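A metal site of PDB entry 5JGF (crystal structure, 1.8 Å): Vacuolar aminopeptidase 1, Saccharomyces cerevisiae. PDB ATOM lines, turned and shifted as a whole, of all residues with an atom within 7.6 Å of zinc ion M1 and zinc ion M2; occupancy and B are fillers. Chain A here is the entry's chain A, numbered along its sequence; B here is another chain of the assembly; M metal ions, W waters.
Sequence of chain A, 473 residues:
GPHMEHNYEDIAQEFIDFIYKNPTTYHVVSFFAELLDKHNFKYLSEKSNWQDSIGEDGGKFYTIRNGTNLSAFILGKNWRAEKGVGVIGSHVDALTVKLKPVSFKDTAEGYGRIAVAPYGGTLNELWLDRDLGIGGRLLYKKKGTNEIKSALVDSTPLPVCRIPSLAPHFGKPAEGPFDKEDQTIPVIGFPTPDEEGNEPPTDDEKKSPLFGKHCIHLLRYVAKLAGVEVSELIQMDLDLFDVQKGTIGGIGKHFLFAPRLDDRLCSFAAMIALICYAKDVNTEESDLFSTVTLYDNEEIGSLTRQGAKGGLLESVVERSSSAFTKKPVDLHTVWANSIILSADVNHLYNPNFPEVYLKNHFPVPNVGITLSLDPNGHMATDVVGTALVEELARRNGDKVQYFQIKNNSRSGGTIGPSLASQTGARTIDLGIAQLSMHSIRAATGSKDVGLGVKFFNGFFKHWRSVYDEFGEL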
ATOM      1  N   SER A  90       5.265  27.505   1.526  1.00  0.00           N
ATOM      2  CA  SER A  90       4.985  26.858   2.804  1.00  0.00           C
ATOM      3  C   SER A  90       6.310  26.479   3.451  1.00  0.00           C
ATOM      4  O   SER A  90       7.367  26.588   2.825  1.00  0.00           O
ATOM      5  CB  SER A  90       4.154  25.587   2.600  1.00  0.00           C
ATOM      6  OG  SER A  90       2.903  25.870   1.994  1.00  0.00           O
ATOM      7  N   HIS A  91       6.280  26.048   4.713  1.00  0.00           N
ATOM      8  CA  HIS A  91       7.528  25.642   5.354  1.00  0.00           C
ATOM      9  C   HIS A  91       7.507  24.162   5.710  1.00  0.00           C
ATOM     10  O   HIS A  91       6.470  23.602   6.063  1.00  0.00           O
ATOM     11  CB  HIS A  91       7.864  26.537   6.568  1.00  0.00           C
ATOM     12  CG  HIS A  91       6.953  26.394   7.752  1.00  0.00           C
ATOM     13  ND1 HIS A  91       7.177  25.478   8.760  1.00  0.00           N
ATOM     14  CD2 HIS A  91       5.877  27.127   8.128  1.00  0.00           C
ATOM     15  CE1 HIS A  91       6.276  25.659   9.707  1.00  0.00           C
ATOM     16  NE2 HIS A  91       5.474  26.649   9.351  1.00  0.00           N
ATOM     17  N   ASP A  93       9.982  22.793   7.865  1.00  0.00           N
ATOM     18  CA  ASP A  93      10.596  22.538   9.154  1.00  0.00           C
ATOM     19  C   ASP A  93       9.461  22.492  10.171  1.00  0.00           C
ATOM     20  O   ASP A  93       8.420  23.111   9.970  1.00  0.00           O
ATOM     21  CB  ASP A  93      11.603  23.633   9.540  1.00  0.00           C
ATOM     22  CG  ASP A  93      10.953  24.996   9.727  1.00  0.00           C
ATOM     23  OD1 ASP A  93      11.239  25.645  10.754  1.00  0.00           O
ATOM     24  OD2 ASP A  93      10.197  25.431   8.836  1.00  0.00           O
ATOM     25  N   ALA A  94       9.644  21.725  11.230  1.00  0.00           N
ATOM     26  CA  ALA A  94       8.630  21.627  12.275  1.00  0.00           C
ATOM     27  C   ALA A  94       9.346  21.590  13.616  1.00  0.00           C
ATOM     28  O   ALA A  94      10.518  21.224  13.686  1.00  0.00           O
ATOM     29  CB  ALA A  94       7.815  20.347  12.086  1.00  0.00           C
ATOM     30  N   LEU A  95       8.651  21.999  14.675  1.00  0.00           N
ATOM     31  CA  LEU A  95       9.257  21.970  15.991  1.00  0.00           C
ATOM     32  C   LEU A  95       9.816  20.582  16.248  1.00  0.00           C
ATOM     33  O   LEU A  95       9.151  19.577  15.965  1.00  0.00           O
ATOM     34  CB  LEU A  95       8.226  22.317  17.072  1.00  0.00           C
ATOM     35  CG  LEU A  95       8.255  23.764  17.582  1.00  0.00           C
ATOM     36  CD1 LEU A  95       8.074  24.727  16.419  1.00  0.00           C
ATOM     37  CD2 LEU A  95       7.167  23.948  18.632  1.00  0.00           C
ATOM     38  N   LEU A 261       2.193  18.614  12.130  1.00  0.00           N
ATOM     39  CA  LEU A 261       1.238  19.123  11.133  1.00  0.00           C
ATOM     40  C   LEU A 261       1.668  20.512  10.626  1.00  0.00           C
ATOM     41  O   LEU A 261       1.519  20.823   9.454  1.00  0.00           O
ATOM     42  CB  LEU A 261      -0.173  19.199  11.739  1.00  0.00           C
ATOM     43  CG  LEU A 261      -0.883  17.893  12.094  1.00  0.00           C
ATOM     44  CD1 LEU A 261      -2.343  18.186  12.466  1.00  0.00           C
ATOM     45  CD2 LEU A 261      -0.840  16.948  10.897  1.00  0.00           C
ATOM     46  N   ASP A 262       2.179  21.332  11.529  1.00  0.00           N
ATOM     47  CA  ASP A 262       2.646  22.668  11.187  1.00  0.00           C
ATOM     48  C   ASP A 262       4.109  22.572  10.711  1.00  0.00           C
ATOM     49  O   ASP A 262       4.987  22.252  11.507  1.00  0.00           O
ATOM     50  CB  ASP A 262       2.577  23.543  12.468  1.00  0.00           C
ATOM     51  CG  ASP A 262       3.108  24.955  12.273  1.00  0.00           C
ATOM     52  OD1 ASP A 262       3.359  25.345  11.124  1.00  0.00           O
ATOM     53  OD2 ASP A 262       3.266  25.704  13.262  1.00  0.00           O
ATOM     54  N   ASP A 263       4.406  22.765   9.417  1.00  0.00           N
ATOM     55  CA  ASP A 263       3.444  23.122   8.368  1.00  0.00           C
ATOM     56  C   ASP A 263       3.475  22.077   7.230  1.00  0.00           C
ATOM     57  O   ASP A 263       3.256  22.394   6.066  1.00  0.00           O
ATOM     58  CB  ASP A 263       3.790  24.537   7.862  1.00  0.00           C
ATOM     59  CG  ASP A 263       2.856  25.055   6.777  1.00  0.00           C
ATOM     60  OD1 ASP A 263       1.636  24.780   6.808  1.00  0.00           O
ATOM     61  OD2 ASP A 263       3.331  25.779   5.869  1.00  0.00           O
ATOM     62  N   ARG A 264       3.769  20.814   7.564  1.00  0.00           N
ATOM     63  CA  ARG A 264       3.847  19.771   6.555  1.00  0.00           C
ATOM     64  C   ARG A 264       2.459  19.418   6.033  1.00  0.00           C
ATOM     65  O   ARG A 264       2.316  18.766   4.999  1.00  0.00           O
ATOM     66  CB  ARG A 264       4.557  18.547   7.140  1.00  0.00           C
ATOM     67  CG  ARG A 264       6.052  18.834   7.322  1.00  0.00           C
ATOM     68  CD  ARG A 264       6.775  17.876   8.244  1.00  0.00           C
ATOM     69  NE  ARG A 264       8.121  18.400   8.505  1.00  0.00           N
ATOM     70  CZ  ARG A 264       9.043  17.801   9.244  1.00  0.00           C
ATOM     71  NH1 ARG A 264       8.773  16.634   9.809  1.00  0.00           N
ATOM     72  NH2 ARG A 264      10.223  18.381   9.433  1.00  0.00           N
ATOM     73  N   GLU A 298      11.219  28.314   9.285  1.00  0.00           N
ATOM     74  CA  GLU A 298      10.180  29.298   9.559  1.00  0.00           C
ATOM     75  C   GLU A 298       9.970  29.394  11.075  1.00  0.00           C
ATOM     76  O   GLU A 298       9.684  30.462  11.618  1.00  0.00           O
ATOM     77  CB  GLU A 298       8.865  28.902   8.877  1.00  0.00           C
ATOM     78  CG  GLU A 298       7.712  29.914   9.033  1.00  0.00           C
ATOM     79  CD  GLU A 298       7.087  29.938  10.420  1.00  0.00           C
ATOM     80  OE1 GLU A 298       7.071  28.881  11.096  1.00  0.00           O
ATOM     81  OE2 GLU A 298       6.581  31.009  10.827  1.00  0.00           O
ATOM     82  N   GLU A 299      10.130  28.255  11.748  1.00  0.00           N
ATOM     83  CA  GLU A 299       9.931  28.191  13.191  1.00  0.00           C
ATOM     84  C   GLU A 299      10.999  28.950  13.985  1.00  0.00           C
ATOM     85  O   GLU A 299      10.842  29.131  15.194  1.00  0.00           O
ATOM     86  CB  GLU A 299       9.858  26.728  13.649  1.00  0.00           C
ATOM     87  CG  GLU A 299       8.682  25.937  13.038  1.00  0.00           C
ATOM     88  CD  GLU A 299       7.311  26.446  13.481  1.00  0.00           C
ATOM     89  OE1 GLU A 299       7.240  27.530  14.104  1.00  0.00           O
ATOM     90  OE2 GLU A 299       6.302  25.767  13.197  1.00  0.00           O
ATOM     91  N   ALA A 343       0.968  29.667   2.423  1.00  0.00           N
ATOM     92  CA  ALA A 343       0.199  28.625   3.076  1.00  0.00           C
ATOM     93  C   ALA A 343       0.846  28.077   4.332  1.00  0.00           C
ATOM     94  O   ALA A 343       1.804  27.314   4.280  1.00  0.00           O
ATOM     95  CB  ALA A 343      -0.069  27.480   2.084  1.00  0.00           C
ATOM     96  N   ASP A 344       0.305  28.491   5.474  1.00  0.00           N
ATOM     97  CA  ASP A 344       0.799  28.037   6.766  1.00  0.00           C
ATOM     98  C   ASP A 344      -0.442  27.740   7.590  1.00  0.00           C
ATOM     99  O   ASP A 344      -1.415  28.489   7.561  1.00  0.00           O
ATOM    100  CB  ASP A 344       1.638  29.134   7.445  1.00  0.00           C
ATOM    101  CG  ASP A 344       2.537  28.581   8.540  1.00  0.00           C
ATOM    102  OD1 ASP A 344       2.373  27.384   8.893  1.00  0.00           O
ATOM    103  OD2 ASP A 344       3.402  29.326   9.040  1.00  0.00           O
ATOM    104  N   VAL A 345      -0.419  26.618   8.308  1.00  0.00           N
ATOM    105  CA  VAL A 345      -1.561  26.224   9.119  1.00  0.00           C
ATOM    106  C   VAL A 345      -1.962  27.330  10.097  1.00  0.00           C
ATOM    107  O   VAL A 345      -1.109  28.068  10.599  1.00  0.00           O
ATOM    108  CB  VAL A 345      -1.268  24.932   9.915  1.00  0.00           C
ATOM    109  CG1 VAL A 345      -1.056  23.758   8.966  1.00  0.00           C
ATOM    110  CG2 VAL A 345      -0.031  25.128  10.791  1.00  0.00           C
ATOM    111  N   ASN A 346      -3.257  27.479  10.328  1.00  0.00           N
ATOM    112  CA  ASN A 346      -3.752  28.446  11.283  1.00  0.00           C
ATOM    113  C   ASN A 346      -4.539  27.698  12.342  1.00  0.00           C
ATOM    114  O   ASN A 346      -4.557  26.462  12.341  1.00  0.00           O
ATOM    115  CB  ASN A 346      -4.601  29.548  10.626  1.00  0.00           C
ATOM    116  CG  ASN A 346      -5.344  29.066   9.412  1.00  0.00           C
ATOM    117  OD1 ASN A 346      -5.944  27.999   9.420  1.00  0.00           O
ATOM    118  ND2 ASN A 346      -5.333  29.869   8.346  1.00  0.00           N
ATOM    119  N   GLY A 413       3.280  34.313  13.631  1.00  0.00           N
ATOM    120  CA  GLY A 413       3.751  34.894  12.394  1.00  0.00           C
ATOM    121  C   GLY A 413       3.871  33.877  11.279  1.00  0.00           C
ATOM    122  O   GLY A 413       3.684  32.680  11.503  1.00  0.00           O
ATOM    123  N   THR A 414       4.184  34.344  10.081  1.00  0.00           N
ATOM    124  CA  THR A 414       4.354  33.465   8.927  1.00  0.00           C
ATOM    125  C   THR A 414       5.403  34.087   8.011  1.00  0.00           C
ATOM    126  O   THR A 414       5.934  35.161   8.297  1.00  0.00           O
ATOM    127  CB  THR A 414       3.052  33.320   8.105  1.00  0.00           C
ATOM    128  OG1 THR A 414       2.789  34.558   7.432  1.00  0.00           O
ATOM    129  CG2 THR A 414       1.878  32.961   9.001  1.00  0.00           C
ATOM    130  N   ILE A 415       5.697  33.403   6.905  1.00  0.00           N
ATOM    131  CA  ILE A 415       6.663  33.914   5.938  1.00  0.00           C
ATOM    132  C   ILE A 415       5.976  34.883   4.977  1.00  0.00           C
ATOM    133  O   ILE A 415       6.630  35.482   4.117  1.00  0.00           O
ATOM    134  CB  ILE A 415       7.256  32.774   5.075  1.00  0.00           C
ATOM    135  CG1 ILE A 415       6.142  32.101   4.274  1.00  0.00           C
ATOM    136  CG2 ILE A 415       7.986  31.770   5.971  1.00  0.00           C
ATOM    137  CD1 ILE A 415       6.629  30.982   3.358  1.00  0.00           C
ATOM    138  N   GLN A 434      -5.742  23.881  12.161  1.00  0.00           N
ATOM    139  CA  GLN A 434      -5.488  22.701  12.985  1.00  0.00           C
ATOM    140  C   GLN A 434      -5.604  23.043  14.464  1.00  0.00           C
ATOM    141  O   GLN A 434      -5.517  24.202  14.866  1.00  0.00           O
ATOM    142  CB  GLN A 434      -4.073  22.173  12.721  1.00  0.00           C
ATOM    143  CG  GLN A 434      -2.969  23.093  13.237  1.00  0.00           C
ATOM    144  CD  GLN A 434      -1.612  22.412  13.298  1.00  0.00           C
ATOM    145  OE1 GLN A 434      -0.852  22.426  12.329  1.00  0.00           O
ATOM    146  NE2 GLN A 434      -1.320  21.807  14.441  1.00  0.00           N
ATOM    147  N   MET A 437      -1.628  23.517  17.656  1.00  0.00           N
ATOM    148  CA  MET A 437      -0.446  23.845  16.887  1.00  0.00           C
ATOM    149  C   MET A 437       0.762  23.878  17.835  1.00  0.00           C
ATOM    150  O   MET A 437       0.659  24.371  18.964  1.00  0.00           O
ATOM    151  CB  MET A 437      -0.614  25.212  16.204  1.00  0.00           C
ATOM    152  CG  MET A 437       0.356  25.464  15.069  1.00  0.00           C
ATOM    153  SD  MET A 437       0.136  27.117  14.378  1.00  0.00           S
ATOM    154  CE  MET A 437      -1.524  26.970  13.710  1.00  0.00           C
ATOM    155  N   HIS A 438       1.882  23.322  17.377  1.00  0.00           N
ATOM    156  CA  HIS A 438       3.132  23.240  18.115  1.00  0.00           C
ATOM    157  C   HIS A 438       3.200  22.181  19.210  1.00  0.00           C
ATOM    158  O   HIS A 438       4.190  22.081  19.934  1.00  0.00           O
ATOM    159  CB  HIS A 438       3.536  24.611  18.675  1.00  0.00           C
ATOM    160  CG  HIS A 438       4.042  25.559  17.631  1.00  0.00           C
ATOM    161  ND1 HIS A 438       4.672  26.746  17.925  1.00  0.00           N
ATOM    162  CD2 HIS A 438       4.007  25.484  16.277  1.00  0.00           C
ATOM    163  CE1 HIS A 438       5.009  27.362  16.811  1.00  0.00           C
ATOM    164  NE2 HIS A 438       4.622  26.620  15.788  1.00  0.00           N
ATOM    165  N   HIS B 169       0.656  30.011  20.872  1.00  0.00           N
ATOM    166  CA  HIS B 169       0.554  31.296  20.182  1.00  0.00           C
ATOM    167  C   HIS B 169      -0.380  32.266  20.903  1.00  0.00           C
ATOM    168  O   HIS B 169      -0.216  33.485  20.811  1.00  0.00           O
ATOM    169  CB  HIS B 169       0.020  31.082  18.756  1.00  0.00           C
ATOM    170  CG  HIS B 169       0.851  30.141  17.937  1.00  0.00           C
ATOM    171  ND1 HIS B 169       1.017  28.816  18.282  1.00  0.00           N
ATOM    172  CD2 HIS B 169       1.563  30.335  16.801  1.00  0.00           C
ATOM    173  CE1 HIS B 169       1.797  28.236  17.388  1.00  0.00           C
ATOM    174  NE2 HIS B 169       2.148  29.132  16.478  1.00  0.00           N
HETATM  175 ZN    ZN M   1       3.726  27.224  10.503  1.00  0.00          ZN
HETATM  176 ZN    ZN M   2       4.723  26.925  13.687  1.00  0.00          ZN
HETATM  177  O   HOH W   1       4.766  28.152  12.149  1.00  0.00           O
HETATM  178  O   HOH W   2       1.830  27.993  11.591  1.00  0.00           O
HETATM  179  O   HOH W   3       3.508  29.598  14.070  1.00  0.00           O
HETATM  180  O   HOH W   4       3.601  30.258  11.457  1.00  0.00           O
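Asp 263 touches zinc ion M1.
Glu 298 touches zinc ion M1 (OE1 to ZN, 3.8 Å).
Of the 22 residues printed, 5 come within 4 Å of zinc ion M1.
Within 4 Å of zinc ion M2: Asp 262, Glu 299 and His 438.
Zinc ion M2 is bound by OD2 of Asp 262 (1.9 Å), water W1 (2.0 Å), OE2 of Glu 299 (2.0 Å) and NE2 of His 438 (2.1 Å).
Zinc ion M2 has four donor atoms within binding distance.
Slightly farther from zinc ion M2 lies the side-chain carboxylate (OE1) of Glu 299 (2.6 Å).
Zinc ion M1 is bound by OD1 of Asp 262 (2.0 Å), OD1 of Asp 344 (2.1 Å), water W1 (2.2 Å), NE2 of His 91 (2.2 Å), water W2 (2.3 Å) and OD2 of Asp 344 (2.6 Å).
Zinc ion M1 has six donor atoms within binding distance.
Water W2 bridges the backbone carbonyl oxygen (O) of Val 345 (3.1 Å) and the side-chain sulfur (SD) of Met 437 (3.4 Å).
Water W1 bridges OE1 of Glu 298 (2.6 Å) and OE1 of Glu 299 (3.2 Å).
Water W4 lies within hydrogen-bond range of the backbone carbonyl oxygen of Gly 413 (2.4 Å) and the side-chain carboxylate of Glu 298 (3.1 Å).
OE1 of Gln 434 lies within hydrogen-bond range of N of Asp 262, at 3.3 Å.
OD1 of Asp 93 lies within hydrogen-bond range of N of Glu 299 (3.0 Å).
OD2 of Asp 263 lies within hydrogen-bond range of N of His 91 (3.2 Å).
A ring nitrogen (NE2) of His 91 sits close to the side-chain carboxylate of Glu 298 (3.3 Å).
ND1 of His 91 is in hydrogen-bond range of O of Asp 93, 2.9 Å away.
The side-chain carboxylate (OD1) of Asp 263 lies within hydrogen-bond range of the backbone NH (N) of Val 345 (3.1 Å).
The side-chain carboxylate of Asp 263 sits close to the backbone carbonyl oxygen of Ala 343.
The backbone NH (N) of Glu 298 lies within hydrogen-bond range of the side-chain carboxylate (OD1) of Asp 93, at 3.0 Å.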
